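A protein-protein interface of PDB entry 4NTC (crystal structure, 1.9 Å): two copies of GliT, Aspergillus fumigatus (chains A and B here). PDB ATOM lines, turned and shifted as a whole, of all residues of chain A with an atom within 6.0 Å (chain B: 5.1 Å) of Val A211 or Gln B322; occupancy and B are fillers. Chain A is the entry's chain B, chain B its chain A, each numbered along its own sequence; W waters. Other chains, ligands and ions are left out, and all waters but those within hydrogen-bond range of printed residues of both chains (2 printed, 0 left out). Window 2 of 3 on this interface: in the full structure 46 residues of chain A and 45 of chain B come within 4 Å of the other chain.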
ATOM      1  N   HIS A 176      -3.920 -15.308  10.392  1.00  0.00           N
ATOM      2  CA  HIS A 176      -3.034 -14.694   9.394  1.00  0.00           C
ATOM      3  C   HIS A 176      -1.574 -15.016   9.708  1.00  0.00           C
ATOM      4  O   HIS A 176      -0.838 -15.443   8.820  1.00  0.00           O
ATOM      5  CB  HIS A 176      -3.278 -13.172   9.327  1.00  0.00           C
ATOM      6  CG  HIS A 176      -2.290 -12.410   8.486  1.00  0.00           C
ATOM      7  ND1 HIS A 176      -2.353 -12.363   7.109  1.00  0.00           N
ATOM      8  CD2 HIS A 176      -1.241 -11.625   8.839  1.00  0.00           C
ATOM      9  CE1 HIS A 176      -1.376 -11.600   6.650  1.00  0.00           C
ATOM     10  NE2 HIS A 176      -0.688 -11.140   7.679  1.00  0.00           N
ATOM     11  N   ARG A 179      -0.857 -19.011   9.566  1.00  0.00           N
ATOM     12  CA  ARG A 179      -0.721 -19.496   8.192  1.00  0.00           C
ATOM     13  C   ARG A 179       0.595 -19.066   7.549  1.00  0.00           C
ATOM     14  O   ARG A 179       1.148 -19.786   6.716  1.00  0.00           O
ATOM     15  CB  ARG A 179      -1.931 -19.093   7.351  1.00  0.00           C
ATOM     16  CG  ARG A 179      -3.137 -19.951   7.692  1.00  0.00           C
ATOM     17  CD  ARG A 179      -4.459 -19.417   7.185  1.00  0.00           C
ATOM     18  NE  ARG A 179      -5.525 -20.325   7.605  1.00  0.00           N
ATOM     19  CZ  ARG A 179      -6.826 -20.104   7.445  1.00  0.00           C
ATOM     20  NH1 ARG A 179      -7.260 -18.988   6.871  1.00  0.00           N
ATOM     21  NH2 ARG A 179      -7.701 -21.010   7.865  1.00  0.00           N
ATOM     22  N   MET A 180       1.098 -17.900   7.950  1.00  0.00           N
ATOM     23  CA  MET A 180       2.431 -17.462   7.553  1.00  0.00           C
ATOM     24  C   MET A 180       3.517 -18.317   8.205  1.00  0.00           C
ATOM     25  O   MET A 180       4.500 -18.673   7.558  1.00  0.00           O
ATOM     26  CB  MET A 180       2.641 -15.983   7.893  1.00  0.00           C
ATOM     27  CG  MET A 180       1.878 -15.021   6.988  1.00  0.00           C
ATOM     28  SD  MET A 180       2.313 -13.297   7.303  1.00  0.00           S
ATOM     29  CE  MET A 180       3.951 -13.209   6.587  1.00  0.00           C
ATOM     30  N   ALA A 181       3.332 -18.642   9.486  1.00  0.00           N
ATOM     31  CA  ALA A 181       4.269 -19.491  10.219  1.00  0.00           C
ATOM     32  C   ALA A 181       4.241 -20.935   9.712  1.00  0.00           C
ATOM     33  O   ALA A 181       5.245 -21.645   9.810  1.00  0.00           O
ATOM     34  CB  ALA A 181       3.973 -19.443  11.711  1.00  0.00           C
ATOM     35  N   ARG A 183       4.252 -21.756   6.703  1.00  0.00           N
ATOM     36  CA  ARG A 183       5.182 -21.805   5.584  1.00  0.00           C
ATOM     37  C   ARG A 183       6.569 -22.226   6.058  1.00  0.00           C
ATOM     38  O   ARG A 183       7.374 -22.723   5.269  1.00  0.00           O
ATOM     39  CB  ARG A 183       5.272 -20.446   4.875  1.00  0.00           C
ATOM     40  CG  ARG A 183       3.941 -19.882   4.374  1.00  0.00           C
ATOM     41  CD  ARG A 183       3.322 -20.722   3.261  1.00  0.00           C
ATOM     42  NE  ARG A 183       4.119 -20.697   2.035  1.00  0.00           N
ATOM     43  CZ  ARG A 183       3.842 -21.395   0.938  1.00  0.00           C
ATOM     44  NH1 ARG A 183       2.778 -22.189   0.892  1.00  0.00           N
ATOM     45  NH2 ARG A 183       4.632 -21.299  -0.121  1.00  0.00           N
ATOM     46  N   ALA A 206     -10.821 -21.222  11.761  1.00  0.00           N
ATOM     47  CA  ALA A 206      -9.938 -22.018  10.910  1.00  0.00           C
ATOM     48  C   ALA A 206     -10.681 -23.217  10.333  1.00  0.00           C
ATOM     49  O   ALA A 206     -10.658 -23.448   9.124  1.00  0.00           O
ATOM     50  CB  ALA A 206      -8.715 -22.475  11.692  1.00  0.00           C
ATOM     51  N   SER A 209     -13.160 -22.168   7.635  1.00  0.00           N
ATOM     52  CA  SER A 209     -12.592 -21.388   6.531  1.00  0.00           C
ATOM     53  C   SER A 209     -12.383 -22.265   5.287  1.00  0.00           C
ATOM     54  O   SER A 209     -12.388 -23.494   5.399  1.00  0.00           O
ATOM     55  CB  SER A 209     -11.263 -20.770   6.962  1.00  0.00           C
ATOM     56  OG  SER A 209     -10.257 -21.765   7.071  1.00  0.00           O
ATOM     57  N   PRO A 210     -12.196 -21.643   4.100  1.00  0.00           N
ATOM     58  CA  PRO A 210     -11.961 -22.435   2.884  1.00  0.00           C
ATOM     59  C   PRO A 210     -10.770 -23.400   2.956  1.00  0.00           C
ATOM     60  O   PRO A 210     -10.841 -24.485   2.379  1.00  0.00           O
ATOM     61  CB  PRO A 210     -11.716 -21.366   1.811  1.00  0.00           C
ATOM     62  CG  PRO A 210     -12.505 -20.195   2.287  1.00  0.00           C
ATOM     63  CD  PRO A 210     -12.366 -20.210   3.787  1.00  0.00           C
ATOM     64  N   VAL A 211      -9.701 -23.022   3.658  1.00  0.00           N
ATOM     65  CA  VAL A 211      -8.486 -23.856   3.693  1.00  0.00           C
ATOM     66  C   VAL A 211      -8.413 -24.833   4.871  1.00  0.00           C
ATOM     67  O   VAL A 211      -7.652 -25.798   4.829  1.00  0.00           O
ATOM     68  CB  VAL A 211      -7.176 -23.029   3.589  1.00  0.00           C
ATOM     69  CG1 VAL A 211      -7.031 -22.410   2.209  1.00  0.00           C
ATOM     70  CG2 VAL A 211      -7.105 -21.959   4.664  1.00  0.00           C
ATOM     71  N   GLY A 212      -9.205 -24.593   5.909  1.00  0.00           N
ATOM     72  CA  GLY A 212      -9.257 -25.510   7.045  1.00  0.00           C
ATOM     73  C   GLY A 212      -8.217 -25.223   8.110  1.00  0.00           C
ATOM     74  O   GLY A 212      -7.522 -24.204   8.062  1.00  0.00           O
ATOM     75  N   ALA A 213      -8.110 -26.138   9.071  1.00  0.00           N
ATOM     76  CA  ALA A 213      -7.264 -25.949  10.248  1.00  0.00           C
ATOM     77  C   ALA A 213      -6.072 -26.903  10.299  1.00  0.00           C
ATOM     78  O   ALA A 213      -5.449 -27.064  11.351  1.00  0.00           O
ATOM     79  CB  ALA A 213      -8.101 -26.088  11.516  1.00  0.00           C
ATOM     80  N   SER A 214      -5.749 -27.531   9.171  1.00  0.00           N
ATOM     81  CA  SER A 214      -4.673 -28.521   9.148  1.00  0.00           C
ATOM     82  C   SER A 214      -3.306 -27.911   9.493  1.00  0.00           C
ATOM     83  O   SER A 214      -2.912 -26.881   8.940  1.00  0.00           O
ATOM     84  CB  SER A 214      -4.646 -29.268   7.809  1.00  0.00           C
ATOM     85  OG  SER A 214      -3.506 -30.111   7.723  1.00  0.00           O
ATOM     86  N   GLN B  36       8.147 -15.703   1.825  1.00  0.00           N
ATOM     87  CA  GLN B  36       7.166 -16.664   2.307  1.00  0.00           C
ATOM     88  C   GLN B  36       7.126 -17.938   1.452  1.00  0.00           C
ATOM     89  O   GLN B  36       6.156 -18.706   1.500  1.00  0.00           O
ATOM     90  CB  GLN B  36       5.794 -15.989   2.411  1.00  0.00           C
ATOM     91  CG  GLN B  36       5.614 -15.228   3.718  1.00  0.00           C
ATOM     92  CD  GLN B  36       5.148 -16.131   4.838  1.00  0.00           C
ATOM     93  OE1 GLN B  36       5.924 -16.499   5.722  1.00  0.00           O
ATOM     94  NE2 GLN B  36       3.874 -16.510   4.797  1.00  0.00           N
ATOM     95  N   HIS B  38       6.669 -18.459  -1.610  1.00  0.00           N
ATOM     96  CA  HIS B  38       5.695 -18.525  -2.687  1.00  0.00           C
ATOM     97  C   HIS B  38       6.374 -18.450  -4.042  1.00  0.00           C
ATOM     98  O   HIS B  38       7.400 -17.789  -4.197  1.00  0.00           O
ATOM     99  CB  HIS B  38       4.603 -17.465  -2.526  1.00  0.00           C
ATOM    100  CG  HIS B  38       3.630 -17.784  -1.433  1.00  0.00           C
ATOM    101  ND1 HIS B  38       2.677 -18.770  -1.556  1.00  0.00           N
ATOM    102  CD2 HIS B  38       3.488 -17.276  -0.183  1.00  0.00           C
ATOM    103  CE1 HIS B  38       1.978 -18.847  -0.437  1.00  0.00           C
ATOM    104  NE2 HIS B  38       2.447 -17.948   0.412  1.00  0.00           N
ATOM    105  N   LEU B 317      -1.183 -10.613  -1.619  1.00  0.00           N
ATOM    106  CA  LEU B 317      -1.075 -11.889  -2.339  1.00  0.00           C
ATOM    107  C   LEU B 317      -0.860 -13.061  -1.386  1.00  0.00           C
ATOM    108  O   LEU B 317      -1.540 -14.082  -1.488  1.00  0.00           O
ATOM    109  CB  LEU B 317       0.067 -11.832  -3.351  1.00  0.00           C
ATOM    110  CG  LEU B 317      -0.141 -11.026  -4.638  1.00  0.00           C
ATOM    111  CD1 LEU B 317       1.208 -10.588  -5.188  1.00  0.00           C
ATOM    112  CD2 LEU B 317      -0.912 -11.839  -5.669  1.00  0.00           C
ATOM    113  N   VAL B 318       0.088 -12.904  -0.463  1.00  0.00           N
ATOM    114  CA  VAL B 318       0.361 -13.921   0.558  1.00  0.00           C
ATOM    115  C   VAL B 318      -0.907 -14.218   1.354  1.00  0.00           C
ATOM    116  O   VAL B 318      -1.251 -15.384   1.563  1.00  0.00           O
ATOM    117  CB  VAL B 318       1.525 -13.491   1.486  1.00  0.00           C
ATOM    118  CG1 VAL B 318       1.559 -14.322   2.764  1.00  0.00           C
ATOM    119  CG2 VAL B 318       2.849 -13.603   0.751  1.00  0.00           C
ATOM    120  N   ALA B 319      -1.609 -13.164   1.770  1.00  0.00           N
ATOM    121  CA  ALA B 319      -2.877 -13.310   2.490  1.00  0.00           C
ATOM    122  C   ALA B 319      -3.899 -14.139   1.701  1.00  0.00           C
ATOM    123  O   ALA B 319      -4.485 -15.070   2.245  1.00  0.00           O
ATOM    124  CB  ALA B 319      -3.452 -11.945   2.856  1.00  0.00           C
ATOM    125  N   GLN B 320      -4.092 -13.801   0.424  1.00  0.00           N
ATOM    126  CA  GLN B 320      -5.045 -14.506  -0.431  1.00  0.00           C
ATOM    127  C   GLN B 320      -4.610 -15.951  -0.679  1.00  0.00           C
ATOM    128  O   GLN B 320      -5.415 -16.872  -0.540  1.00  0.00           O
ATOM    129  CB  GLN B 320      -5.232 -13.778  -1.769  1.00  0.00           C
ATOM    130  CG  GLN B 320      -6.062 -12.503  -1.688  1.00  0.00           C
ATOM    131  CD  GLN B 320      -6.379 -11.904  -3.054  1.00  0.00           C
ATOM    132  OE1 GLN B 320      -6.149 -12.521  -4.096  1.00  0.00           O
ATOM    133  NE2 GLN B 320      -6.914 -10.694  -3.048  1.00  0.00           N
ATOM    134  N   LEU B 321      -3.338 -16.140  -1.033  1.00  0.00           N
ATOM    135  CA  LEU B 321      -2.799 -17.474  -1.330  1.00  0.00           C
ATOM    136  C   LEU B 321      -2.941 -18.433  -0.156  1.00  0.00           C
ATOM    137  O   LEU B 321      -3.177 -19.630  -0.349  1.00  0.00           O
ATOM    138  CB  LEU B 321      -1.333 -17.392  -1.773  1.00  0.00           C
ATOM    139  CG  LEU B 321      -1.065 -16.770  -3.153  1.00  0.00           C
ATOM    140  CD1 LEU B 321       0.383 -16.317  -3.261  1.00  0.00           C
ATOM    141  CD2 LEU B 321      -1.423 -17.727  -4.285  1.00  0.00           C
ATOM    142  N   GLN B 322      -2.815 -17.907   1.059  1.00  0.00           N
ATOM    143  CA  GLN B 322      -2.863 -18.744   2.260  1.00  0.00           C
ATOM    144  C   GLN B 322      -4.269 -18.923   2.830  1.00  0.00           C
ATOM    145  O   GLN B 322      -4.496 -19.824   3.641  1.00  0.00           O
ATOM    146  CB  GLN B 322      -1.900 -18.206   3.321  1.00  0.00           C
ATOM    147  CG  GLN B 322      -0.441 -18.345   2.902  1.00  0.00           C
ATOM    148  CD  GLN B 322       0.542 -17.637   3.816  1.00  0.00           C
ATOM    149  OE1 GLN B 322       1.715 -17.479   3.473  1.00  0.00           O
ATOM    150  NE2 GLN B 322       0.074 -17.204   4.979  1.00  0.00           N
ATOM    151  N   ALA B 323      -5.205 -18.076   2.399  1.00  0.00           N
ATOM    152  CA  ALA B 323      -6.591 -18.129   2.879  1.00  0.00           C
ATOM    153  C   ALA B 323      -7.532 -18.804   1.882  1.00  0.00           C
ATOM    154  O   ALA B 323      -8.652 -19.170   2.232  1.00  0.00           O
ATOM    155  CB  ALA B 323      -7.093 -16.730   3.212  1.00  0.00           C
ATOM    156  N   GLN B 324      -7.072 -18.965   0.645  1.00  0.00           N
ATOM    157  CA  GLN B 324      -7.904 -19.532  -0.412  1.00  0.00           C
ATOM    158  C   GLN B 324      -7.428 -20.921  -0.818  1.00  0.00           C
ATOM    159  O   GLN B 324      -6.226 -21.158  -0.977  1.00  0.00           O
ATOM    160  CB  GLN B 324      -7.960 -18.590  -1.617  1.00  0.00           C
ATOM    161  CG  GLN B 324      -8.554 -17.224  -1.288  1.00  0.00           C
ATOM    162  CD  GLN B 324      -8.400 -16.216  -2.414  1.00  0.00           C
ATOM    163  OE1 GLN B 324      -8.090 -16.577  -3.553  1.00  0.00           O
ATOM    164  NE2 GLN B 324      -8.616 -14.942  -2.101  1.00  0.00           N
ATOM    165  N   ALA B 325      -8.385 -21.835  -0.964  1.00  0.00           N
ATOM    166  CA  ALA B 325      -8.110 -23.232  -1.290  1.00  0.00           C
ATOM    167  C   ALA B 325      -7.390 -23.392  -2.626  1.00  0.00           C
ATOM    168  O   ALA B 325      -7.736 -22.744  -3.618  1.00  0.00           O
ATOM    169  CB  ALA B 325      -9.398 -24.044  -1.278  1.00  0.00           C
HETATM  170  O   HOH W   1      -9.289 -19.353   4.879  1.00  0.00           O
HETATM  171  O   HOH W   2      -1.681 -15.517   6.080  1.00  0.00           O
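Water W2 bridges the side-chain amide nitrogen (NE2) of Gln B322 (2.7 Å) and the backbone carbonyl oxygen (O) of His A176 (2.9 Å). Water W1 lies within hydrogen-bond range of O of Ala B323 (2.7 Å), NH1 of Arg A179 (2.9 Å) and OG of Ser A209 (3.4 Å).
No position is printed for both chains. Of the 12 pairs that touch across the chains among the printed residues, none has its exchanged pair printed and touching as well.
Among the printed residues, merely in contact across the chains: Arg A183 with His B38 (3.4 Å), Arg A183 with Gln B322 (3.4 Å), Pro A210 with Ala B323 (3.8 Å), Pro A210 with Ala B325 (3.96 Å), Val A211 with Gln B322 (3.5 Å), Val A211 with Ala B323 (3.6 Å), Val A211 with Gln B324 (3.4 Å) and Val A211 with Ala B325 (3.5 Å).
Of the printed residues of chain B, Arg A179 touches Gln B322 (3.2 Å). Printed residues of chain B within 4 Å of Met A180: Gln B36 and Gln B322. Val A211 touches four residues of chain B. Of the printed residues of chain A, His B38 touches Arg A183 (3.4 Å). Leu B317 touches none of the printed residues of chain A. Val B318 touches none of the printed residues of chain A. Gln B322 touches just these residues of chain A: Arg A179, Met A180, Arg A183 and Val A211. Of the printed residues of chain A, Gln B324 touches Val A211. The nearest printed residue of chain B that does not touch Val A211 is Leu B321 (5.4 Å). The nearest residue of chain A that does not touch Gln B322 is His A176 (4.3 Å).
The side-chain amide nitrogen of Gln B36 sits at hydrogen-bond distance from the side-chain amide oxygen of Gln B322, 2.7 Å away. The guanidinium group (NH2) of Arg A179 is in hydrogen-bond range of the backbone carbonyl oxygen (O) of Gly A212 (3.2 Å). NE2 of His B38 sits at hydrogen-bond distance from OE1 of Gln B322 (3.2 Å). A ring nitrogen (NE2) of His A176 is in hydrogen-bond range of the side-chain sulfur of Met A180 (3.7 Å). The guanidinium group (NH2) of Arg A179 lies within hydrogen-bond range of the side-chain hydroxyl (OG) of Ser A209, 2.8 Å away.
The backbone carbonyl oxygen (O) of Gln B36 sits at hydrogen-bond distance from the guanidinium group (NE) of Arg A183, 2.9 Å away. The side-chain amide nitrogen (NE2) of Gln B322 lies close to the backbone NH (N) of Met A180 (3.2 Å). NE2 of Gln B322 sits close to O of Arg A179. The backbone carbonyl oxygen (O) of Met A180 lies close to the side-chain amide oxygen (OE1) of Gln B36 (3.2 Å).
Printed residues of chain A that touch a printed residue of chain B: Arg A179, Met A180, Arg A183, Pro A210 and Val A211. Hydrophobic or aromatic side chains of chain A within 4 Å of the printed part of chain B: Met A180, Pro A210 and Val A211. Of the 11 printed residues of chain B, 6 touch a printed residue of chain A. Among the printed residues, no Asp or Glu carboxylate lies within 4 Å of a Lys or Arg side-chain nitrogen of the other chain.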
